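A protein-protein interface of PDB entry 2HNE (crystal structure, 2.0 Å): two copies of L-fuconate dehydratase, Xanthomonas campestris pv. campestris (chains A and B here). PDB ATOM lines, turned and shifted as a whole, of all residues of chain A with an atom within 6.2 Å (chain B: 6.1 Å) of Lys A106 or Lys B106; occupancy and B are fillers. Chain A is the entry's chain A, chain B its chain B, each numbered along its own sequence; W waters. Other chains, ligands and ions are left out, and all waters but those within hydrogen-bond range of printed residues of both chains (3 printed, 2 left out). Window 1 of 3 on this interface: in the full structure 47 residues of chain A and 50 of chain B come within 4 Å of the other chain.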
ATOM      1  N   LEU A 102      10.280  19.863 -27.897  1.00  0.00           N
ATOM      2  CA  LEU A 102      10.811  20.960 -27.085  1.00  0.00           C
ATOM      3  C   LEU A 102       9.997  21.154 -25.800  1.00  0.00           C
ATOM      4  O   LEU A 102      10.379  21.927 -24.919  1.00  0.00           O
ATOM      5  CB  LEU A 102      10.830  22.259 -27.894  1.00  0.00           C
ATOM      6  CG  LEU A 102      11.889  22.433 -29.000  1.00  0.00           C
ATOM      7  CD1 LEU A 102      13.265  22.210 -28.415  1.00  0.00           C
ATOM      8  CD2 LEU A 102      11.657  21.452 -30.131  1.00  0.00           C
ATOM      9  N   GLY A 103       8.877  20.450 -25.694  1.00  0.00           N
ATOM     10  CA  GLY A 103       8.048  20.543 -24.503  1.00  0.00           C
ATOM     11  C   GLY A 103       7.971  19.197 -23.800  1.00  0.00           C
ATOM     12  O   GLY A 103       8.919  18.792 -23.135  1.00  0.00           O
ATOM     13  N   PRO A 104       6.855  18.469 -23.928  1.00  0.00           N
ATOM     14  CA  PRO A 104       5.652  18.829 -24.686  1.00  0.00           C
ATOM     15  C   PRO A 104       4.645  19.690 -23.906  1.00  0.00           C
ATOM     16  O   PRO A 104       4.404  19.472 -22.718  1.00  0.00           O
ATOM     17  CB  PRO A 104       5.064  17.468 -25.049  1.00  0.00           C
ATOM     18  CG  PRO A 104       5.358  16.672 -23.823  1.00  0.00           C
ATOM     19  CD  PRO A 104       6.803  17.052 -23.515  1.00  0.00           C
ATOM     20  N   GLU A 105       4.063  20.664 -24.595  1.00  0.00           N
ATOM     21  CA  GLU A 105       3.055  21.533 -24.009  1.00  0.00           C
ATOM     22  C   GLU A 105       3.475  22.179 -22.686  1.00  0.00           C
ATOM     23  O   GLU A 105       2.728  22.188 -21.702  1.00  0.00           O
ATOM     24  CB  GLU A 105       1.743  20.743 -23.850  1.00  0.00           C
ATOM     25  CG  GLU A 105       1.150  20.323 -25.196  1.00  0.00           C
ATOM     26  CD  GLU A 105      -0.150  19.545 -25.073  1.00  0.00           C
ATOM     27  OE1 GLU A 105      -1.084  20.039 -24.404  1.00  0.00           O
ATOM     28  OE2 GLU A 105      -0.243  18.441 -25.660  1.00  0.00           O
ATOM     29  N   LYS A 106       4.686  22.721 -22.682  1.00  0.00           N
ATOM     30  CA  LYS A 106       5.220  23.409 -21.518  1.00  0.00           C
ATOM     31  C   LYS A 106       6.364  24.313 -21.967  1.00  0.00           C
ATOM     32  O   LYS A 106       6.895  24.166 -23.070  1.00  0.00           O
ATOM     33  CB  LYS A 106       5.724  22.398 -20.496  1.00  0.00           C
ATOM     34  CG  LYS A 106       6.927  21.603 -20.973  1.00  0.00           C
ATOM     35  CD  LYS A 106       7.237  20.465 -20.035  1.00  0.00           C
ATOM     36  CE  LYS A 106       6.298  19.286 -20.274  1.00  0.00           C
ATOM     37  NZ  LYS A 106       6.737  18.120 -19.479  1.00  0.00           N
ATOM     38  N   GLY A 107       6.728  25.266 -21.120  1.00  0.00           N
ATOM     39  CA  GLY A 107       7.825  26.162 -21.445  1.00  0.00           C
ATOM     40  C   GLY A 107       7.681  27.102 -22.630  1.00  0.00           C
ATOM     41  O   GLY A 107       6.594  27.315 -23.168  1.00  0.00           O
ATOM     42  N   VAL A 108       8.821  27.662 -23.027  1.00  0.00           N
ATOM     43  CA  VAL A 108       8.935  28.617 -24.121  1.00  0.00           C
ATOM     44  C   VAL A 108       8.183  28.268 -25.400  1.00  0.00           C
ATOM     45  O   VAL A 108       7.443  29.093 -25.922  1.00  0.00           O
ATOM     46  CB  VAL A 108      10.427  28.846 -24.479  1.00  0.00           C
ATOM     47  CG1 VAL A 108      10.551  29.588 -25.810  1.00  0.00           C
ATOM     48  CG2 VAL A 108      11.108  29.635 -23.364  1.00  0.00           C
ATOM     49  N   MET A 109       8.375  27.052 -25.906  1.00  0.00           N
ATOM     50  CA  MET A 109       7.720  26.648 -27.143  1.00  0.00           C
ATOM     51  C   MET A 109       6.198  26.647 -27.015  1.00  0.00           C
ATOM     52  O   MET A 109       5.505  27.080 -27.918  1.00  0.00           O
ATOM     53  CB  MET A 109       8.217  25.266 -27.578  1.00  0.00           C
ATOM     54  CG  MET A 109       7.920  24.945 -29.026  1.00  0.00           C
ATOM     55  SD  MET A 109       8.681  26.131 -30.169  1.00  0.00           S
ATOM     56  CE  MET A 109      10.148  25.259 -30.644  1.00  0.00           C
ATOM     57  N   HIS A 110       5.674  26.175 -25.891  1.00  0.00           N
ATOM     58  CA  HIS A 110       4.230  26.149 -25.717  1.00  0.00           C
ATOM     59  C   HIS A 110       3.673  27.575 -25.577  1.00  0.00           C
ATOM     60  O   HIS A 110       2.610  27.889 -26.109  1.00  0.00           O
ATOM     61  CB  HIS A 110       3.864  25.320 -24.493  1.00  0.00           C
ATOM     62  CG  HIS A 110       2.438  24.875 -24.475  1.00  0.00           C
ATOM     63  ND1 HIS A 110       1.829  24.311 -25.577  1.00  0.00           N
ATOM     64  CD2 HIS A 110       1.517  24.852 -23.482  1.00  0.00           C
ATOM     65  CE1 HIS A 110       0.599  23.951 -25.260  1.00  0.00           C
ATOM     66  NE2 HIS A 110       0.383  24.267 -23.995  1.00  0.00           N
ATOM     67  N   MET A 111       4.395  28.438 -24.866  1.00  0.00           N
ATOM     68  CA  MET A 111       3.929  29.806 -24.708  1.00  0.00           C
ATOM     69  C   MET A 111       3.943  30.525 -26.054  1.00  0.00           C
ATOM     70  O   MET A 111       3.093  31.378 -26.308  1.00  0.00           O
ATOM     71  CB  MET A 111       4.772  30.563 -23.677  1.00  0.00           C
ATOM     72  CG  MET A 111       4.561  30.065 -22.265  1.00  0.00           C
ATOM     73  SD  MET A 111       5.078  31.248 -21.008  1.00  0.00           S
ATOM     74  CE  MET A 111       6.822  31.104 -21.140  1.00  0.00           C
ATOM     75  N   PRO A 279       5.279  24.764  -8.754  1.00  0.00           N
ATOM     76  CA  PRO A 279       4.093  24.695  -9.614  1.00  0.00           C
ATOM     77  C   PRO A 279       3.908  23.339 -10.305  1.00  0.00           C
ATOM     78  O   PRO A 279       2.911  23.124 -10.988  1.00  0.00           O
ATOM     79  CB  PRO A 279       4.337  25.814 -10.614  1.00  0.00           C
ATOM     80  CG  PRO A 279       5.804  25.765 -10.785  1.00  0.00           C
ATOM     81  CD  PRO A 279       6.316  25.611  -9.374  1.00  0.00           C
ATOM     82  N   ASP A 280       4.881  22.449 -10.129  1.00  0.00           N
ATOM     83  CA  ASP A 280       4.841  21.109 -10.712  1.00  0.00           C
ATOM     84  C   ASP A 280       4.469  20.077  -9.657  1.00  0.00           C
ATOM     85  O   ASP A 280       4.182  18.927  -9.982  1.00  0.00           O
ATOM     86  CB  ASP A 280       6.210  20.718 -11.288  1.00  0.00           C
ATOM     87  CG  ASP A 280       6.676  21.658 -12.381  1.00  0.00           C
ATOM     88  OD1 ASP A 280       5.810  22.208 -13.092  1.00  0.00           O
ATOM     89  OD2 ASP A 280       7.907  21.837 -12.539  1.00  0.00           O
ATOM     90  N   HIS A 302       1.460  29.621 -13.107  1.00  0.00           N
ATOM     91  CA  HIS A 302       2.607  28.988 -13.757  1.00  0.00           C
ATOM     92  C   HIS A 302       2.340  27.549 -14.179  1.00  0.00           C
ATOM     93  O   HIS A 302       3.237  26.865 -14.653  1.00  0.00           O
ATOM     94  CB  HIS A 302       3.822  29.018 -12.830  1.00  0.00           C
ATOM     95  CG  HIS A 302       4.766  30.143 -13.112  1.00  0.00           C
ATOM     96  ND1 HIS A 302       4.370  31.306 -13.734  1.00  0.00           N
ATOM     97  CD2 HIS A 302       6.083  30.295 -12.837  1.00  0.00           C
ATOM     98  CE1 HIS A 302       5.400  32.126 -13.831  1.00  0.00           C
ATOM     99  NE2 HIS A 302       6.452  31.537 -13.293  1.00  0.00           N
ATOM    100  N   THR A 303       1.113  27.082 -13.981  1.00  0.00           N
ATOM    101  CA  THR A 303       0.743  25.718 -14.359  1.00  0.00           C
ATOM    102  C   THR A 303       0.873  25.584 -15.878  1.00  0.00           C
ATOM    103  O   THR A 303       0.246  26.325 -16.627  1.00  0.00           O
ATOM    104  CB  THR A 303      -0.680  25.434 -13.909  1.00  0.00           C
ATOM    105  OG1 THR A 303      -0.748  25.615 -12.491  1.00  0.00           O
ATOM    106  CG2 THR A 303      -1.090  24.011 -14.255  1.00  0.00           C
ATOM    107  N   GLN A 304       1.691  24.625 -16.312  1.00  0.00           N
ATOM    108  CA  GLN A 304       1.993  24.404 -17.723  1.00  0.00           C
ATOM    109  C   GLN A 304       0.896  24.098 -18.732  1.00  0.00           C
ATOM    110  O   GLN A 304       0.941  24.605 -19.855  1.00  0.00           O
ATOM    111  CB  GLN A 304       3.067  23.320 -17.842  1.00  0.00           C
ATOM    112  CG  GLN A 304       2.668  21.983 -17.224  1.00  0.00           C
ATOM    113  CD  GLN A 304       3.861  21.103 -16.927  1.00  0.00           C
ATOM    114  OE1 GLN A 304       4.076  20.078 -17.577  1.00  0.00           O
ATOM    115  NE2 GLN A 304       4.655  21.505 -15.942  1.00  0.00           N
ATOM    116  N   ASN A 305      -0.070  23.264 -18.369  1.00  0.00           N
ATOM    117  CA  ASN A 305      -1.124  22.915 -19.326  1.00  0.00           C
ATOM    118  C   ASN A 305      -2.341  22.308 -18.637  1.00  0.00           C
ATOM    119  O   ASN A 305      -2.332  22.089 -17.438  1.00  0.00           O
ATOM    120  CB  ASN A 305      -0.569  21.924 -20.358  1.00  0.00           C
ATOM    121  CG  ASN A 305      -0.007  20.679 -19.707  1.00  0.00           C
ATOM    122  OD1 ASN A 305      -0.652  20.074 -18.846  1.00  0.00           O
ATOM    123  ND2 ASN A 305       1.202  20.287 -20.109  1.00  0.00           N
ATOM    124  N   LEU B 102      10.686  31.556 -17.785  1.00  0.00           N
ATOM    125  CA  LEU B 102      10.453  30.858 -19.046  1.00  0.00           C
ATOM    126  C   LEU B 102      10.201  29.372 -18.826  1.00  0.00           C
ATOM    127  O   LEU B 102      10.001  28.620 -19.785  1.00  0.00           O
ATOM    128  CB  LEU B 102      11.641  31.057 -19.998  1.00  0.00           C
ATOM    129  CG  LEU B 102      11.868  32.513 -20.415  1.00  0.00           C
ATOM    130  CD1 LEU B 102      12.967  32.592 -21.457  1.00  0.00           C
ATOM    131  CD2 LEU B 102      10.580  33.083 -20.987  1.00  0.00           C
ATOM    132  N   GLY B 103      10.203  28.970 -17.556  1.00  0.00           N
ATOM    133  CA  GLY B 103       9.957  27.587 -17.186  1.00  0.00           C
ATOM    134  C   GLY B 103       8.881  27.537 -16.111  1.00  0.00           C
ATOM    135  O   GLY B 103       7.700  27.697 -16.405  1.00  0.00           O
ATOM    136  N   PRO B 104       9.258  27.329 -14.846  1.00  0.00           N
ATOM    137  CA  PRO B 104      10.640  27.139 -14.419  1.00  0.00           C
ATOM    138  C   PRO B 104      11.015  25.662 -14.435  1.00  0.00           C
ATOM    139  O   PRO B 104      10.179  24.798 -14.186  1.00  0.00           O
ATOM    140  CB  PRO B 104      10.630  27.710 -13.008  1.00  0.00           C
ATOM    141  CG  PRO B 104       9.307  27.239 -12.508  1.00  0.00           C
ATOM    142  CD  PRO B 104       8.371  27.494 -13.678  1.00  0.00           C
ATOM    143  N   GLU B 105      12.277  25.392 -14.739  1.00  0.00           N
ATOM    144  CA  GLU B 105      12.807  24.035 -14.762  1.00  0.00           C
ATOM    145  C   GLU B 105      11.997  23.069 -15.640  1.00  0.00           C
ATOM    146  O   GLU B 105      11.588  21.993 -15.200  1.00  0.00           O
ATOM    147  CB  GLU B 105      12.926  23.509 -13.326  1.00  0.00           C
ATOM    148  CG  GLU B 105      13.757  24.437 -12.406  1.00  0.00           C
ATOM    149  CD  GLU B 105      14.072  23.830 -11.042  1.00  0.00           C
ATOM    150  OE1 GLU B 105      14.494  24.583 -10.134  1.00  0.00           O
ATOM    151  OE2 GLU B 105      13.910  22.603 -10.872  1.00  0.00           O
ATOM    152  N   LYS B 106      11.786  23.474 -16.889  1.00  0.00           N
ATOM    153  CA  LYS B 106      11.055  22.671 -17.868  1.00  0.00           C
ATOM    154  C   LYS B 106      11.170  23.329 -19.232  1.00  0.00           C
ATOM    155  O   LYS B 106      11.503  24.513 -19.333  1.00  0.00           O
ATOM    156  CB  LYS B 106       9.571  22.566 -17.504  1.00  0.00           C
ATOM    157  CG  LYS B 106       8.794  23.856 -17.710  1.00  0.00           C
ATOM    158  CD  LYS B 106       7.373  23.772 -17.166  1.00  0.00           C
ATOM    159  CE  LYS B 106       7.365  23.667 -15.648  1.00  0.00           C
ATOM    160  NZ  LYS B 106       5.982  23.736 -15.111  1.00  0.00           N
ATOM    161  N   GLY B 107      10.909  22.562 -20.284  1.00  0.00           N
ATOM    162  CA  GLY B 107      10.951  23.120 -21.621  1.00  0.00           C
ATOM    163  C   GLY B 107      12.313  23.529 -22.142  1.00  0.00           C
ATOM    164  O   GLY B 107      13.342  23.182 -21.573  1.00  0.00           O
ATOM    165  N   VAL B 108      12.297  24.288 -23.232  1.00  0.00           N
ATOM    166  CA  VAL B 108      13.504  24.760 -23.910  1.00  0.00           C
ATOM    167  C   VAL B 108      14.564  25.431 -23.029  1.00  0.00           C
ATOM    168  O   VAL B 108      15.737  25.046 -23.056  1.00  0.00           O
ATOM    169  CB  VAL B 108      13.120  25.723 -25.053  1.00  0.00           C
ATOM    170  CG1 VAL B 108      14.373  26.364 -25.669  1.00  0.00           C
ATOM    171  CG2 VAL B 108      12.349  24.962 -26.122  1.00  0.00           C
ATOM    172  N   MET B 109      14.161  26.435 -22.259  1.00  0.00           N
ATOM    173  CA  MET B 109      15.115  27.142 -21.404  1.00  0.00           C
ATOM    174  C   MET B 109      15.834  26.212 -20.428  1.00  0.00           C
ATOM    175  O   MET B 109      17.041  26.341 -20.230  1.00  0.00           O
ATOM    176  CB  MET B 109      14.413  28.278 -20.642  1.00  0.00           C
ATOM    177  CG  MET B 109      15.364  29.354 -20.092  1.00  0.00           C
ATOM    178  SD  MET B 109      16.604  29.914 -21.299  1.00  0.00           S
ATOM    179  CE  MET B 109      15.749  31.118 -22.179  1.00  0.00           C
ATOM    180  N   HIS B 110      15.120  25.253 -19.844  1.00  0.00           N
ATOM    181  CA  HIS B 110      15.758  24.350 -18.895  1.00  0.00           C
ATOM    182  C   HIS B 110      16.726  23.401 -19.586  1.00  0.00           C
ATOM    183  O   HIS B 110      17.813  23.136 -19.063  1.00  0.00           O
ATOM    184  CB  HIS B 110      14.719  23.546 -18.120  1.00  0.00           C
ATOM    185  CG  HIS B 110      15.259  22.879 -16.892  1.00  0.00           C
ATOM    186  ND1 HIS B 110      15.949  23.564 -15.914  1.00  0.00           N
ATOM    187  CD2 HIS B 110      15.160  21.601 -16.456  1.00  0.00           C
ATOM    188  CE1 HIS B 110      16.249  22.738 -14.928  1.00  0.00           C
ATOM    189  NE2 HIS B 110      15.782  21.540 -15.231  1.00  0.00           N
ATOM    190  N   MET B 111      16.350  22.881 -20.756  1.00  0.00           N
ATOM    191  CA  MET B 111      17.264  21.981 -21.448  1.00  0.00           C
ATOM    192  C   MET B 111      18.505  22.762 -21.878  1.00  0.00           C
ATOM    193  O   MET B 111      19.611  22.213 -21.922  1.00  0.00           O
ATOM    194  CB  MET B 111      16.587  21.319 -22.654  1.00  0.00           C
ATOM    195  CG  MET B 111      15.530  20.308 -22.241  1.00  0.00           C
ATOM    196  SD  MET B 111      15.064  19.223 -23.593  1.00  0.00           S
ATOM    197  CE  MET B 111      14.117  20.330 -24.553  1.00  0.00           C
ATOM    198  N   PRO B 279       3.566  12.670 -20.406  1.00  0.00           N
ATOM    199  CA  PRO B 279       4.674  12.684 -19.453  1.00  0.00           C
ATOM    200  C   PRO B 279       4.427  13.566 -18.218  1.00  0.00           C
ATOM    201  O   PRO B 279       5.251  13.613 -17.307  1.00  0.00           O
ATOM    202  CB  PRO B 279       5.844  13.180 -20.298  1.00  0.00           C
ATOM    203  CG  PRO B 279       5.185  14.138 -21.224  1.00  0.00           C
ATOM    204  CD  PRO B 279       3.942  13.358 -21.652  1.00  0.00           C
ATOM    205  N   ASP B 280       3.304  14.273 -18.195  1.00  0.00           N
ATOM    206  CA  ASP B 280       2.977  15.119 -17.053  1.00  0.00           C
ATOM    207  C   ASP B 280       1.913  14.456 -16.192  1.00  0.00           C
ATOM    208  O   ASP B 280       1.649  14.903 -15.072  1.00  0.00           O
ATOM    209  CB  ASP B 280       2.448  16.477 -17.517  1.00  0.00           C
ATOM    210  CG  ASP B 280       3.469  17.255 -18.312  1.00  0.00           C
ATOM    211  OD1 ASP B 280       4.670  17.133 -17.996  1.00  0.00           O
ATOM    212  OD2 ASP B 280       3.075  17.993 -19.244  1.00  0.00           O
ATOM    213  N   HIS B 302      10.974  12.210 -20.965  1.00  0.00           N
ATOM    214  CA  HIS B 302      10.492  13.575 -21.125  1.00  0.00           C
ATOM    215  C   HIS B 302      10.080  14.189 -19.785  1.00  0.00           C
ATOM    216  O   HIS B 302       9.479  15.252 -19.762  1.00  0.00           O
ATOM    217  CB  HIS B 302       9.291  13.626 -22.083  1.00  0.00           C
ATOM    218  CG  HIS B 302       9.665  13.803 -23.520  1.00  0.00           C
ATOM    219  ND1 HIS B 302       8.726  13.941 -24.518  1.00  0.00           N
ATOM    220  CD2 HIS B 302      10.871  13.863 -24.130  1.00  0.00           C
ATOM    221  CE1 HIS B 302       9.337  14.075 -25.681  1.00  0.00           C
ATOM    222  NE2 HIS B 302      10.639  14.030 -25.475  1.00  0.00           N
ATOM    223  N   THR B 303      10.386  13.519 -18.678  1.00  0.00           N
ATOM    224  CA  THR B 303      10.020  14.047 -17.368  1.00  0.00           C
ATOM    225  C   THR B 303      10.846  15.311 -17.188  1.00  0.00           C
ATOM    226  O   THR B 303      12.071  15.279 -17.248  1.00  0.00           O
ATOM    227  CB  THR B 303      10.304  13.028 -16.258  1.00  0.00           C
ATOM    228  OG1 THR B 303       9.558  11.830 -16.521  1.00  0.00           O
ATOM    229  CG2 THR B 303       9.876  13.581 -14.896  1.00  0.00           C
ATOM    230  N   GLN B 304      10.158  16.425 -16.967  1.00  0.00           N
ATOM    231  CA  GLN B 304      10.809  17.732 -16.892  1.00  0.00           C
ATOM    232  C   GLN B 304      11.853  18.020 -15.830  1.00  0.00           C
ATOM    233  O   GLN B 304      12.816  18.729 -16.102  1.00  0.00           O
ATOM    234  CB  GLN B 304       9.734  18.818 -16.837  1.00  0.00           C
ATOM    235  CG  GLN B 304       8.833  18.673 -15.647  1.00  0.00           C
ATOM    236  CD  GLN B 304       7.567  19.454 -15.805  1.00  0.00           C
ATOM    237  OE1 GLN B 304       7.269  20.348 -15.012  1.00  0.00           O
ATOM    238  NE2 GLN B 304       6.802  19.125 -16.841  1.00  0.00           N
ATOM    239  N   ASN B 305      11.659  17.503 -14.625  1.00  0.00           N
ATOM    240  CA  ASN B 305      12.611  17.745 -13.550  1.00  0.00           C
ATOM    241  C   ASN B 305      12.465  16.751 -12.419  1.00  0.00           C
ATOM    242  O   ASN B 305      11.581  15.904 -12.430  1.00  0.00           O
ATOM    243  CB  ASN B 305      12.448  19.165 -12.997  1.00  0.00           C
ATOM    244  CG  ASN B 305      11.029  19.468 -12.540  1.00  0.00           C
ATOM    245  OD1 ASN B 305      10.443  18.726 -11.764  1.00  0.00           O
ATOM    246  ND2 ASN B 305      10.480  20.584 -13.019  1.00  0.00           N
HETATM  247  O   HOH W   1       9.286  17.694 -20.626  1.00  0.00           O
HETATM  248  O   HOH W   2       5.235  26.359 -16.177  1.00  0.00           O
HETATM  249  O   HOH W   3       3.016  22.944 -13.996  1.00  0.00           O
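Water W2 lies within hydrogen-bond range of the backbone carbonyl oxygen (O) of His A302 (2.6 Å), the backbone carbonyl oxygen (O) of Gly B103 (2.8 Å) and the side-chain amino group (NZ) of Lys B106 (2.9 Å). Water W1 lies within hydrogen-bond range of the backbone carbonyl oxygen of His B302 (2.6 Å), the backbone carbonyl oxygen of Gly A103 (2.8 Å) and the side-chain amino group of Lys A106 (2.8 Å). Water W3 lies within hydrogen-bond range of NE2 of Gln A304 (2.9 Å), O of Pro A279 (3.0 Å), OD1 of Asp A280 (3.0 Å) and NZ of Lys B106 (3.3 Å).
Leu A102 touches Val B108, and with the chains exchanged Val A108 touches Leu B102. Lys A106 touches Asp B280, and with the chains exchanged Asp A280 touches Lys B106. Lys A106 touches Gln B304, and with the chains exchanged Gln A304 touches Lys B106. Asp A280 touches Gln B304, and with the chains exchanged Gln A304 touches Asp B280. 16 positions are printed for both chains.
Among the printed residues, pairs that only touch across the chains: Leu A102 with Gly B107, Pro A104 with Pro B279, Pro A104 with His B302, Lys A106 with Lys B106, Lys A106 with His B302, Gly A107 with Leu B102, Val A108 with Leu B102 and His A302 with Pro B104.
The side-chain amide nitrogen (ND2) of Asn A305 sits at hydrogen-bond distance from the backbone carbonyl oxygen (O) of Glu A105 (2.9 Å). OD1 of Asp A280 is in hydrogen-bond range of NE2 of Gln A304, at 3.2 Å. The backbone carbonyl oxygen (O) of Glu B105 is in hydrogen-bond range of the side-chain amide nitrogen (ND2) of Asn B305, at 2.8 Å. The side-chain amide nitrogen (NE2) of Gln B304 is in hydrogen-bond range of the side-chain carboxylate (OD1) of Asp B280 (3.1 Å).
Of the 16 printed residues of chain B, 10 touch a printed residue of chain A. Hydrophobic or aromatic side chains of chain B within 4 Å of the printed part of chain A: Leu B102, Pro B104, Val B108, Pro B279 and His B302. Along chain B the printed residues that touch a printed residue of chain A span positions 102 to 305. Of the 16 printed residues of chain A, 9 touch a printed residue of chain B. Printed residues of chain A that touch a printed residue of chain B: Leu A102, Pro A104, Lys A106, Gly A107, Val A108, Asp A280, His A302, Gln A304 and Asn A305. Hydrophobic or aromatic side chains of chain A within 4 Å of the printed part of chain B: Leu A102, Pro A104, Val A108 and His A302. Among the printed residues, 18 pairs touch across the chains.
O of Leu A102 is in hydrogen-bond range of N of Val B108 (3.5 Å). OD1 of Asp B280 is in salt-bridge range of NZ of Lys A106 (2.7 Å). NZ of Lys A106 sits close to NE2 of Gln B304 (2.8 Å). The side-chain carboxylate (OD1) of Asp A280 is in salt-bridge range of the side-chain amino group (NZ) of Lys B106. The side-chain carboxylate (OD2) of Asp A280 lies close to the side-chain amide oxygen (OE1) of Gln B304. The side-chain amide nitrogen of Asn B305 sits at hydrogen-bond distance from the side-chain carboxylate of Asp A280 (2.9 Å). The side-chain amide nitrogen (NE2) of Gln A304 sits close to the side-chain amino group (NZ) of Lys B106 (2.7 Å). OE1 of Gln A304 lies close to OD2 of Asp B280 (2.9 Å). NE2 of Gln B304 is in hydrogen-bond range of OE1 of Gln A304, 3.0 Å away. ND2 of Asn A305 is in hydrogen-bond range of OD2 of Asp B280, 3.1 Å away.
Lys A106 touches just these residues of chain B: Lys B106, Asp B280, His B302 and Gln B304. Of the printed residues of chain B, Val A108 touches Leu B102 (3.6 Å). Met A111 touches none of the printed residues of chain B. Of chain A, only Lys A106 (3.96 Å), Asp A280 (2.5 Å) and Gln A304 (2.7 Å) come within 4 Å of Lys B106. Of the printed residues of chain A, Val B108 touches Leu A102. Of the printed residues of chain A, His B302 touches Pro A104 and Lys A106. The nearest residue of chain B that does not touch Lys A106 is Gly B107 (4.2 Å). The nearest printed residue of chain B that does not touch Gly A107 is Lys B106 (4.2 Å).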
